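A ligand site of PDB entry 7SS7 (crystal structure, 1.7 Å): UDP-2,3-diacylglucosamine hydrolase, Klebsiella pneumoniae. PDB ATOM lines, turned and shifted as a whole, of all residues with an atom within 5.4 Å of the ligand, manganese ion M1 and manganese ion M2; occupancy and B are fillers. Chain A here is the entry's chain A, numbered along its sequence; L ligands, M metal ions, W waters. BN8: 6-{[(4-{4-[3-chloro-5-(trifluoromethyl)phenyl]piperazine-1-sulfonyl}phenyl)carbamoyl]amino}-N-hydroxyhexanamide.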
ATOM      1  N   ASP A   8      14.236  20.196   3.690  1.00  0.00           N
ATOM      2  CA  ASP A   8      12.867  19.919   4.093  1.00  0.00           C
ATOM      3  C   ASP A   8      11.919  19.785   2.894  1.00  0.00           C
ATOM      4  O   ASP A   8      10.779  20.261   2.902  1.00  0.00           O
ATOM      5  CB  ASP A   8      12.385  21.007   5.068  1.00  0.00           C
ATOM      6  CG  ASP A   8      13.199  20.983   6.349  1.00  0.00           C
ATOM      7  OD1 ASP A   8      13.157  19.948   7.037  1.00  0.00           O
ATOM      8  OD2 ASP A   8      13.890  21.965   6.661  1.00  0.00           O
ATOM      9  N   HIS A  10      11.083  16.571   1.958  1.00  0.00           N
ATOM     10  CA  HIS A  10      10.325  15.384   2.410  1.00  0.00           C
ATOM     11  C   HIS A  10       9.756  14.617   1.227  1.00  0.00           C
ATOM     12  O   HIS A  10       8.578  14.233   1.205  1.00  0.00           O
ATOM     13  CB  HIS A  10       9.213  15.769   3.396  1.00  0.00           C
ATOM     14  CG  HIS A  10       9.647  16.744   4.440  1.00  0.00           C
ATOM     15  ND1 HIS A  10       9.247  18.060   4.439  1.00  0.00           N
ATOM     16  CD2 HIS A  10      10.469  16.604   5.520  1.00  0.00           C
ATOM     17  CE1 HIS A  10       9.797  18.688   5.458  1.00  0.00           C
ATOM     18  NE2 HIS A  10      10.548  17.829   6.126  1.00  0.00           N
ATOM     19  N   ASP A  41      16.594  16.358   5.346  1.00  0.00           N
ATOM     20  CA  ASP A  41      15.188  16.070   5.070  1.00  0.00           C
ATOM     21  C   ASP A  41      14.875  16.226   3.587  1.00  0.00           C
ATOM     22  O   ASP A  41      13.821  16.743   3.188  1.00  0.00           O
ATOM     23  CB  ASP A  41      14.257  16.921   5.948  1.00  0.00           C
ATOM     24  CG  ASP A  41      14.208  16.429   7.380  1.00  0.00           C
ATOM     25  OD1 ASP A  41      14.923  15.450   7.697  1.00  0.00           O
ATOM     26  OD2 ASP A  41      13.480  17.023   8.184  1.00  0.00           O
ATOM     27  N   GLU A  44      11.377  11.984   2.904  1.00  0.00           N
ATOM     28  CA  GLU A  44      10.523  11.827   4.092  1.00  0.00           C
ATOM     29  C   GLU A  44      10.943  10.642   4.944  1.00  0.00           C
ATOM     30  O   GLU A  44      10.647  10.611   6.149  1.00  0.00           O
ATOM     31  CB  GLU A  44       9.051  11.686   3.666  1.00  0.00           C
ATOM     32  CG  GLU A  44       8.075  11.310   4.801  1.00  0.00           C
ATOM     33  CD  GLU A  44       7.937  12.337   5.913  1.00  0.00           C
ATOM     34  OE1 GLU A  44       7.189  12.064   6.873  1.00  0.00           O
ATOM     35  OE2 GLU A  44       8.541  13.427   5.845  1.00  0.00           O
ATOM     36  N   ALA A  45      11.640   9.662   4.358  1.00  0.00           N
ATOM     37  CA  ALA A  45      12.081   8.497   5.110  1.00  0.00           C
ATOM     38  C   ALA A  45      13.300   7.918   4.405  1.00  0.00           C
ATOM     39  O   ALA A  45      13.526   8.151   3.212  1.00  0.00           O
ATOM     40  CB  ALA A  45      10.966   7.446   5.204  1.00  0.00           C
ATOM     41  N   TRP A  46      14.124   7.183   5.160  1.00  0.00           N
ATOM     42  CA  TRP A  46      15.233   6.439   4.556  1.00  0.00           C
ATOM     43  C   TRP A  46      15.539   5.256   5.445  1.00  0.00           C
ATOM     44  O   TRP A  46      15.743   5.445   6.654  1.00  0.00           O
ATOM     45  CB  TRP A  46      16.491   7.309   4.401  1.00  0.00           C
ATOM     46  CG  TRP A  46      17.461   6.792   3.361  1.00  0.00           C
ATOM     47  CD1 TRP A  46      18.552   5.993   3.564  1.00  0.00           C
ATOM     48  CD2 TRP A  46      17.427   7.084   1.967  1.00  0.00           C
ATOM     49  NE1 TRP A  46      19.195   5.760   2.356  1.00  0.00           N
ATOM     50  CE2 TRP A  46      18.516   6.426   1.361  1.00  0.00           C
ATOM     51  CE3 TRP A  46      16.559   7.831   1.161  1.00  0.00           C
ATOM     52  CZ2 TRP A  46      18.784   6.509  -0.007  1.00  0.00           C
ATOM     53  CZ3 TRP A  46      16.830   7.920  -0.214  1.00  0.00           C
ATOM     54  CH2 TRP A  46      17.923   7.258  -0.779  1.00  0.00           C
ATOM     55  N   ILE A  47      15.589   4.063   4.868  1.00  0.00           N
ATOM     56  CA  ILE A  47      15.897   2.871   5.650  1.00  0.00           C
ATOM     57  C   ILE A  47      17.187   2.194   5.185  1.00  0.00           C
ATOM     58  O   ILE A  47      17.480   1.081   5.622  1.00  0.00           O
ATOM     59  CB  ILE A  47      14.721   1.865   5.660  1.00  0.00           C
ATOM     60  CG1 ILE A  47      14.382   1.415   4.226  1.00  0.00           C
ATOM     61  CG2 ILE A  47      13.492   2.480   6.365  1.00  0.00           C
ATOM     62  CD1 ILE A  47      13.372   0.295   4.149  1.00  0.00           C
ATOM     63  N   GLY A  78      19.251  15.120   7.531  1.00  0.00           N
ATOM     64  CA  GLY A  78      18.160  15.543   8.391  1.00  0.00           C
ATOM     65  C   GLY A  78      17.773  14.440   9.379  1.00  0.00           C
ATOM     66  O   GLY A  78      18.343  13.359   9.397  1.00  0.00           O
ATOM     67  N   ASN A  79      16.779  14.743  10.214  1.00  0.00           N
ATOM     68  CA  ASN A  79      16.278  13.710  11.116  1.00  0.00           C
ATOM     69  C   ASN A  79      15.431  12.657  10.375  1.00  0.00           C
ATOM     70  O   ASN A  79      15.268  11.548  10.888  1.00  0.00           O
ATOM     71  CB  ASN A  79      15.457  14.341  12.239  1.00  0.00           C
ATOM     72  CG  ASN A  79      14.327  15.172  11.722  1.00  0.00           C
ATOM     73  OD1 ASN A  79      14.541  16.223  11.137  1.00  0.00           O
ATOM     74  ND2 ASN A  79      13.095  14.703  11.925  1.00  0.00           N
ATOM     75  N   ARG A  80      14.890  12.982   9.202  1.00  0.00           N
ATOM     76  CA  ARG A  80      14.136  11.962   8.475  1.00  0.00           C
ATOM     77  C   ARG A  80      15.055  11.028   7.701  1.00  0.00           C
ATOM     78  O   ARG A  80      14.761   9.823   7.574  1.00  0.00           O
ATOM     79  CB  ARG A  80      13.139  12.600   7.486  1.00  0.00           C
ATOM     80  CG  ARG A  80      12.160  13.582   8.122  1.00  0.00           C
ATOM     81  CD  ARG A  80      11.335  12.899   9.229  1.00  0.00           C
ATOM     82  NE  ARG A  80      10.577  11.753   8.713  1.00  0.00           N
ATOM     83  CZ  ARG A  80       9.661  11.113   9.422  1.00  0.00           C
ATOM     84  NH1 ARG A  80       9.355  11.482  10.659  1.00  0.00           N
ATOM     85  NH2 ARG A  80       9.028  10.087   8.870  1.00  0.00           N
ATOM     86  N   PHE A  82      18.593  10.423   8.007  1.00  0.00           N
ATOM     87  CA  PHE A  82      19.929  10.275   8.566  1.00  0.00           C
ATOM     88  C   PHE A  82      20.648   9.013   8.102  1.00  0.00           C
ATOM     89  O   PHE A  82      21.872   8.915   8.262  1.00  0.00           O
ATOM     90  CB  PHE A  82      19.879  10.304  10.115  1.00  0.00           C
ATOM     91  CG  PHE A  82      19.015   9.221  10.744  1.00  0.00           C
ATOM     92  CD1 PHE A  82      17.644   9.435  10.981  1.00  0.00           C
ATOM     93  CD2 PHE A  82      19.574   8.015  11.141  1.00  0.00           C
ATOM     94  CE1 PHE A  82      16.858   8.439  11.581  1.00  0.00           C
ATOM     95  CE2 PHE A  82      18.803   7.017  11.731  1.00  0.00           C
ATOM     96  CZ  PHE A  82      17.438   7.230  11.955  1.00  0.00           C
ATOM     97  N   LEU A  83      19.941   8.038   7.522  1.00  0.00           N
ATOM     98  CA  LEU A  83      20.603   6.826   7.037  1.00  0.00           C
ATOM     99  C   LEU A  83      21.114   6.929   5.608  1.00  0.00           C
ATOM    100  O   LEU A  83      21.642   5.947   5.089  1.00  0.00           O
ATOM    101  CB  LEU A  83      19.684   5.611   7.154  1.00  0.00           C
ATOM    102  CG  LEU A  83      19.411   5.121   8.576  1.00  0.00           C
ATOM    103  CD1 LEU A  83      18.512   3.873   8.543  1.00  0.00           C
ATOM    104  CD2 LEU A  83      20.724   4.821   9.341  1.00  0.00           C
ATOM    105  N   HIS A 114      21.377  21.099   9.634  1.00  0.00           N
ATOM    106  CA  HIS A 114      19.950  20.835   9.455  1.00  0.00           C
ATOM    107  C   HIS A 114      19.122  21.693  10.399  1.00  0.00           C
ATOM    108  O   HIS A 114      18.078  22.225  10.002  1.00  0.00           O
ATOM    109  CB  HIS A 114      19.611  19.347   9.660  1.00  0.00           C
ATOM    110  CG  HIS A 114      18.153  19.062   9.479  1.00  0.00           C
ATOM    111  ND1 HIS A 114      17.468  19.338   8.312  1.00  0.00           N
ATOM    112  CD2 HIS A 114      17.232  18.532  10.329  1.00  0.00           C
ATOM    113  CE1 HIS A 114      16.200  18.999   8.447  1.00  0.00           C
ATOM    114  NE2 HIS A 114      16.028  18.509   9.658  1.00  0.00           N
ATOM    115  N   ASP A 116      18.122  20.566  13.720  1.00  0.00           N
ATOM    116  CA  ASP A 116      17.469  19.883  14.831  1.00  0.00           C
ATOM    117  C   ASP A 116      18.336  19.869  16.088  1.00  0.00           C
ATOM    118  O   ASP A 116      17.796  19.827  17.204  1.00  0.00           O
ATOM    119  CB  ASP A 116      17.080  18.447  14.439  1.00  0.00           C
ATOM    120  CG  ASP A 116      18.260  17.614  13.997  1.00  0.00           C
ATOM    121  OD1 ASP A 116      19.046  18.049  13.130  1.00  0.00           O
ATOM    122  OD2 ASP A 116      18.408  16.493  14.519  1.00  0.00           O
ATOM    123  N   TYR A 125      13.652  14.345  22.304  1.00  0.00           N
ATOM    124  CA  TYR A 125      14.093  14.200  20.932  1.00  0.00           C
ATOM    125  C   TYR A 125      15.600  13.993  20.860  1.00  0.00           C
ATOM    126  O   TYR A 125      16.077  13.118  20.131  1.00  0.00           O
ATOM    127  CB  TYR A 125      13.699  15.406  20.096  1.00  0.00           C
ATOM    128  CG  TYR A 125      14.391  15.358  18.751  1.00  0.00           C
ATOM    129  CD1 TYR A 125      14.022  14.417  17.809  1.00  0.00           C
ATOM    130  CD2 TYR A 125      15.467  16.197  18.461  1.00  0.00           C
ATOM    131  CE1 TYR A 125      14.659  14.333  16.592  1.00  0.00           C
ATOM    132  CE2 TYR A 125      16.128  16.111  17.238  1.00  0.00           C
ATOM    133  CZ  TYR A 125      15.710  15.180  16.313  1.00  0.00           C
ATOM    134  OH  TYR A 125      16.358  15.088  15.093  1.00  0.00           O
ATOM    135  N   PHE A 128      16.571  10.422  21.644  1.00  0.00           N
ATOM    136  CA  PHE A 128      16.281   9.574  20.495  1.00  0.00           C
ATOM    137  C   PHE A 128      17.304   9.786  19.373  1.00  0.00           C
ATOM    138  O   PHE A 128      17.783   8.820  18.763  1.00  0.00           O
ATOM    139  CB  PHE A 128      14.866   9.872  19.995  1.00  0.00           C
ATOM    140  CG  PHE A 128      14.550   9.279  18.655  1.00  0.00           C
ATOM    141  CD1 PHE A 128      14.153   7.966  18.541  1.00  0.00           C
ATOM    142  CD2 PHE A 128      14.656  10.054  17.504  1.00  0.00           C
ATOM    143  CE1 PHE A 128      13.861   7.410  17.300  1.00  0.00           C
ATOM    144  CE2 PHE A 128      14.374   9.511  16.266  1.00  0.00           C
ATOM    145  CZ  PHE A 128      13.970   8.186  16.165  1.00  0.00           C
ATOM    146  N   VAL A 132      19.775   6.844  17.538  1.00  0.00           N
ATOM    147  CA  VAL A 132      19.799   6.458  16.121  1.00  0.00           C
ATOM    148  C   VAL A 132      21.046   6.955  15.397  1.00  0.00           C
ATOM    149  O   VAL A 132      21.295   6.525  14.266  1.00  0.00           O
ATOM    150  CB  VAL A 132      18.537   6.889  15.341  1.00  0.00           C
ATOM    151  CG1 VAL A 132      17.278   6.240  15.936  1.00  0.00           C
ATOM    152  CG2 VAL A 132      18.397   8.423  15.268  1.00  0.00           C
ATOM    153  N   ILE A 137      24.247   0.885  16.531  1.00  0.00           N
ATOM    154  CA  ILE A 137      22.806   0.736  16.366  1.00  0.00           C
ATOM    155  C   ILE A 137      22.443   0.852  14.896  1.00  0.00           C
ATOM    156  O   ILE A 137      21.650   0.056  14.369  1.00  0.00           O
ATOM    157  CB  ILE A 137      22.061   1.763  17.243  1.00  0.00           C
ATOM    158  CG1 ILE A 137      22.324   1.445  18.713  1.00  0.00           C
ATOM    159  CG2 ILE A 137      20.562   1.733  16.933  1.00  0.00           C
ATOM    160  CD1 ILE A 137      21.600   2.374  19.694  1.00  0.00           C
ATOM    161  N   GLN A 138      23.029   1.812  14.177  1.00  0.00           N
ATOM    162  CA  GLN A 138      22.781   1.898  12.744  1.00  0.00           C
ATOM    163  C   GLN A 138      23.204   0.629  12.032  1.00  0.00           C
ATOM    164  O   GLN A 138      22.505   0.146  11.136  1.00  0.00           O
ATOM    165  CB  GLN A 138      23.505   3.110  12.143  1.00  0.00           C
ATOM    166  CG  GLN A 138      22.974   4.443  12.626  1.00  0.00           C
ATOM    167  CD  GLN A 138      23.576   5.582  11.849  1.00  0.00           C
ATOM    168  OE1 GLN A 138      24.438   5.369  10.994  1.00  0.00           O
ATOM    169  NE2 GLN A 138      23.112   6.811  12.123  1.00  0.00           N
ATOM    170  N   PHE A 141      20.584  -2.107  12.613  1.00  0.00           N
ATOM    171  CA  PHE A 141      19.354  -1.852  11.857  1.00  0.00           C
ATOM    172  C   PHE A 141      19.559  -2.131  10.374  1.00  0.00           C
ATOM    173  O   PHE A 141      18.748  -2.808   9.735  1.00  0.00           O
ATOM    174  CB  PHE A 141      18.895  -0.408  12.073  1.00  0.00           C
ATOM    175  CG  PHE A 141      17.686  -0.040  11.244  1.00  0.00           C
ATOM    176  CD1 PHE A 141      16.409  -0.367  11.684  1.00  0.00           C
ATOM    177  CD2 PHE A 141      17.843   0.600  10.021  1.00  0.00           C
ATOM    178  CE1 PHE A 141      15.303  -0.026  10.918  1.00  0.00           C
ATOM    179  CE2 PHE A 141      16.739   0.933   9.249  1.00  0.00           C
ATOM    180  CZ  PHE A 141      15.482   0.619   9.695  1.00  0.00           C
ATOM    181  N   ILE A 152       9.246  -1.878  10.043  1.00  0.00           N
ATOM    182  CA  ILE A 152       9.563  -1.058  11.207  1.00  0.00           C
ATOM    183  C   ILE A 152       9.255   0.394  10.915  1.00  0.00           C
ATOM    184  O   ILE A 152       8.635   1.098  11.723  1.00  0.00           O
ATOM    185  CB  ILE A 152      11.034  -1.246  11.603  1.00  0.00           C
ATOM    186  CG1 ILE A 152      11.288  -2.645  12.175  1.00  0.00           C
ATOM    187  CG2 ILE A 152      11.479  -0.191  12.597  1.00  0.00           C
ATOM    188  CD1 ILE A 152      12.752  -2.924  12.331  1.00  0.00           C
ATOM    189  N   ALA A 153       9.653   0.870   9.733  1.00  0.00           N
ATOM    190  CA  ALA A 153       9.455   2.271   9.385  1.00  0.00           C
ATOM    191  C   ALA A 153       7.976   2.600   9.241  1.00  0.00           C
ATOM    192  O   ALA A 153       7.517   3.659   9.704  1.00  0.00           O
ATOM    193  CB  ALA A 153      10.212   2.601   8.100  1.00  0.00           C
ATOM    194  N   MET A 156       6.437   2.756  12.684  1.00  0.00           N
ATOM    195  CA  MET A 156       6.786   3.980  13.420  1.00  0.00           C
ATOM    196  C   MET A 156       5.970   5.169  12.938  1.00  0.00           C
ATOM    197  O   MET A 156       5.678   6.076  13.719  1.00  0.00           O
ATOM    198  CB  MET A 156       8.287   4.252  13.297  1.00  0.00           C
ATOM    199  CG  MET A 156       9.157   3.402  14.222  1.00  0.00           C
ATOM    200  SD  MET A 156      10.935   3.492  13.926  1.00  0.00           S
ATOM    201  CE  MET A 156      11.329   5.081  14.644  1.00  0.00           C
ATOM    202  N   MET A 172       9.024  21.586  17.091  1.00  0.00           N
ATOM    203  CA  MET A 172       9.914  22.289  18.001  1.00  0.00           C
ATOM    204  C   MET A 172      10.649  23.428  17.296  1.00  0.00           C
ATOM    205  O   MET A 172      10.862  23.390  16.079  1.00  0.00           O
ATOM    206  CB  MET A 172      10.931  21.297  18.578  1.00  0.00           C
ATOM    207  CG  MET A 172      11.721  20.557  17.499  1.00  0.00           C
ATOM    208  SD  MET A 172      12.255  18.887  17.946  1.00  0.00           S
ATOM    209  CE  MET A 172      11.581  17.960  16.573  1.00  0.00           C
ATOM    210  N   HIS A 195      14.757  22.380   9.255  1.00  0.00           N
ATOM    211  CA  HIS A 195      14.133  21.616  10.347  1.00  0.00           C
ATOM    212  C   HIS A 195      12.886  22.259  10.942  1.00  0.00           C
ATOM    213  O   HIS A 195      11.882  21.552  11.141  1.00  0.00           O
ATOM    214  CB  HIS A 195      15.095  21.334  11.502  1.00  0.00           C
ATOM    215  CG  HIS A 195      14.517  20.391  12.508  1.00  0.00           C
ATOM    216  ND1 HIS A 195      14.189  19.088  12.206  1.00  0.00           N
ATOM    217  CD2 HIS A 195      14.172  20.568  13.809  1.00  0.00           C
ATOM    218  CE1 HIS A 195      13.687  18.501  13.270  1.00  0.00           C
ATOM    219  NE2 HIS A 195      13.673  19.370  14.265  1.00  0.00           N
ATOM    220  N   THR A 196      12.919  23.548  11.274  1.00  0.00           N
ATOM    221  CA  THR A 196      11.798  24.126  12.006  1.00  0.00           C
ATOM    222  C   THR A 196      10.641  24.515  11.105  1.00  0.00           C
ATOM    223  O   THR A 196       9.560  24.837  11.609  1.00  0.00           O
ATOM    224  CB  THR A 196      12.262  25.349  12.805  1.00  0.00           C
ATOM    225  OG1 THR A 196      12.752  26.341  11.904  1.00  0.00           O
ATOM    226  CG2 THR A 196      13.372  24.953  13.764  1.00  0.00           C
ATOM    227  N   HIS A 197      10.834  24.512   9.783  1.00  0.00           N
ATOM    228  CA  HIS A 197       9.779  24.799   8.821  1.00  0.00           C
ATOM    229  C   HIS A 197       9.172  26.192   9.025  1.00  0.00           C
ATOM    230  O   HIS A 197       7.983  26.388   8.786  1.00  0.00           O
ATOM    231  CB  HIS A 197       8.680  23.730   8.877  1.00  0.00           C
ATOM    232  CG  HIS A 197       9.142  22.336   8.580  1.00  0.00           C
ATOM    233  ND1 HIS A 197       8.287  21.256   8.549  1.00  0.00           N
ATOM    234  CD2 HIS A 197      10.371  21.847   8.287  1.00  0.00           C
ATOM    235  CE1 HIS A 197       8.965  20.159   8.260  1.00  0.00           C
ATOM    236  NE2 HIS A 197      10.241  20.489   8.105  1.00  0.00           N
HETATM  237  C13 BN8 L   1      10.880   7.427  11.203  1.00  0.00           C
HETATM  238  C15 BN8 L   1      11.515   9.393  12.410  1.00  0.00           C
HETATM  239  C17 BN8 L   1      12.751   8.767  10.436  1.00  0.00           C
HETATM  240  C22 BN8 L   1      11.558  13.875  14.803  1.00  0.00           C
HETATM  241  C24 BN8 L   1      10.755  16.024  13.723  1.00  0.00           C
HETATM  242  C26 BN8 L   1      10.086  15.982  11.283  1.00  0.00           C
HETATM  243  C01 BN8 L   1      16.904   3.565  12.442  1.00  0.00           C
HETATM  244  C02 BN8 L   1      15.550   3.334  12.453  1.00  0.00           C
HETATM  245  C04 BN8 L   1      15.380   4.616  10.325  1.00  0.00           C
HETATM  246  C05 BN8 L   1      14.503   5.794   9.934  1.00  0.00           C
HETATM  247  C07 BN8 L   1      12.558   4.564  10.697  1.00  0.00           C
HETATM  248  C08 BN8 L   1      13.437   3.395  11.110  1.00  0.00           C
HETATM  249  C12 BN8 L   1      11.907   7.678  10.302  1.00  0.00           C
HETATM  250  C14 BN8 L   1      10.678   8.295  12.257  1.00  0.00           C
HETATM  251  C16 BN8 L   1      12.543   9.622  11.504  1.00  0.00           C
HETATM  252  C19 BN8 L   1      11.581  11.701  13.580  1.00  0.00           C
HETATM  253  C23 BN8 L   1      10.361  14.609  14.183  1.00  0.00           C
HETATM  254  C25 BN8 L   1       9.784  16.577  12.669  1.00  0.00           C
HETATM  255  C27 BN8 L   1      10.710  16.975  10.299  1.00  0.00           C
HETATM  256  C31 BN8 L   1      14.945   2.551  13.424  1.00  0.00           C
HETATM  257  C32 BN8 L   1      15.755   1.999  14.394  1.00  0.00           C
HETATM  258  C33 BN8 L   1      17.114   2.226  14.424  1.00  0.00           C
HETATM  259  C34 BN8 L   1      17.685   3.015  13.431  1.00  0.00           C
HETATM  260  C36 BN8 L   1      15.086   1.135  15.462  1.00  0.00           C
HETATM  261  F37 BN8 L   1      14.195   1.909  16.117  1.00  0.00           F
HETATM  262  F38 BN8 L   1      16.040   0.650  16.301  1.00  0.00           F
HETATM  263  F39 BN8 L   1      14.434   0.100  14.879  1.00  0.00           F
HETATM  264  N03 BN8 L   1      14.744   3.910  11.421  1.00  0.00           N
HETATM  265  N06 BN8 L   1      13.153   5.345   9.622  1.00  0.00           N
HETATM  266  N18 BN8 L   1      11.265  10.276  13.527  1.00  0.00           N
HETATM  267  N21 BN8 L   1      11.258  12.458  14.764  1.00  0.00           N
HETATM  268  N29 BN8 L   1      11.578  18.030  10.809  1.00  0.00           N
HETATM  269  O10 BN8 L   1      10.869   5.963   8.567  1.00  0.00           O
HETATM  270  O11 BN8 L   1      12.855   7.139   7.858  1.00  0.00           O
HETATM  271  O20 BN8 L   1      12.105  12.257  12.667  1.00  0.00           O
HETATM  272  O28 BN8 L   1      10.485  16.917   9.114  1.00  0.00           O
HETATM  273  O30 BN8 L   1      12.159  18.953   9.899  1.00  0.00           O
HETATM  274  S09 BN8 L   1      12.148   6.515   8.970  1.00  0.00           S
HETATM  275 CL35 BN8 L   1      19.414   3.340  13.384  1.00  0.00          CL
HETATM  276 MN    MN M   1      11.721  18.678   7.858  1.00  0.00          MN
HETATM  277 MN    MN M   2      13.943  17.862  10.280  1.00  0.00          MN
HETATM  278  O   HOH W   1       8.013   6.588   8.958  1.00  0.00           O
HETATM  279  O   HOH W   2       8.620  15.020   8.018  1.00  0.00           O
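An oxygen (O20) of the ligand lies close to the guanidinium group of Arg 80, 3.5 Å away.
An oxygen (O30) of the ligand sits close to the backbone carbonyl oxygen of His 195, at 2.9 Å.
O11 of the ligand lies within hydrogen-bond range of N of Trp 46, at 3.0 Å.
The side-chain hydroxyl of Tyr 125 sits at hydrogen-bond distance from the side-chain carboxylate of Asp 116, at 2.6 Å.
NE2 of Gln 138 lies within hydrogen-bond range of O of Val 132 (2.8 Å).
The side-chain carboxylate (OE1) of Glu 44 is in salt-bridge range of the guanidinium group (NH2) of Arg 80 (3.4 Å).
The backbone NH (N) of His 195 sits at hydrogen-bond distance from the side-chain carboxylate (OD2) of Asp 8 (2.8 Å).
The side-chain carboxylate (OD1) of Asp 41 is in hydrogen-bond range of the backbone NH (N) of Arg 80 (2.9 Å).
Merely in contact with the ligand: Ala 45, Phe 82, Leu 83, Tyr 125, Val 132, Gln 138, Phe 141, Ile 152, Ala 153, Met 156 and Met 172.
Hydrophobic or aromatic side chains that line the ligand: His 10, Ala 45, Phe 82, Leu 83, Tyr 125, Phe 141, Ile 152, Ala 153, Met 156, Met 172, His 195 and His 197.
Within 4 Å of the ligand: Asp 8, His 10, Asp 41, Ala 45, Trp 46, Asn 79, Arg 80, Phe 82, Leu 83, His 114, Tyr 125, Val 132, Gln 138, Phe 141, Ile 152, Ala 153, Met 156, Met 172, His 195 and His 197.
The nearest printed residue that does not touch manganese ion M2 is His 197 (5.0 Å).
Manganese ion M1 is bound by OD1 of Asp 8 (2.1 Å), O30 of the ligand (2.1 Å), NE2 of His 10 (2.3 Å), NE2 of His 197 (2.4 Å), OD2 of Asp 41 (2.4 Å) and O28 of the ligand (2.5 Å).
Manganese ion M1 has six donor atoms within binding distance.
Manganese ion M2 is bound by OD1 of Asn 79 (1.9 Å), O30 of the ligand (2.1 Å), NE2 of His 114 (2.3 Å), ND1 of His 195 (2.3 Å) and OD2 of Asp 41 (2.3 Å).
Manganese ion M2 has five donor atoms within binding distance.
Water W1 bridges an oxygen (O10) of the ligand (2.9 Å) and the backbone carbonyl oxygen (O) of Ala 153 (3.1 Å).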
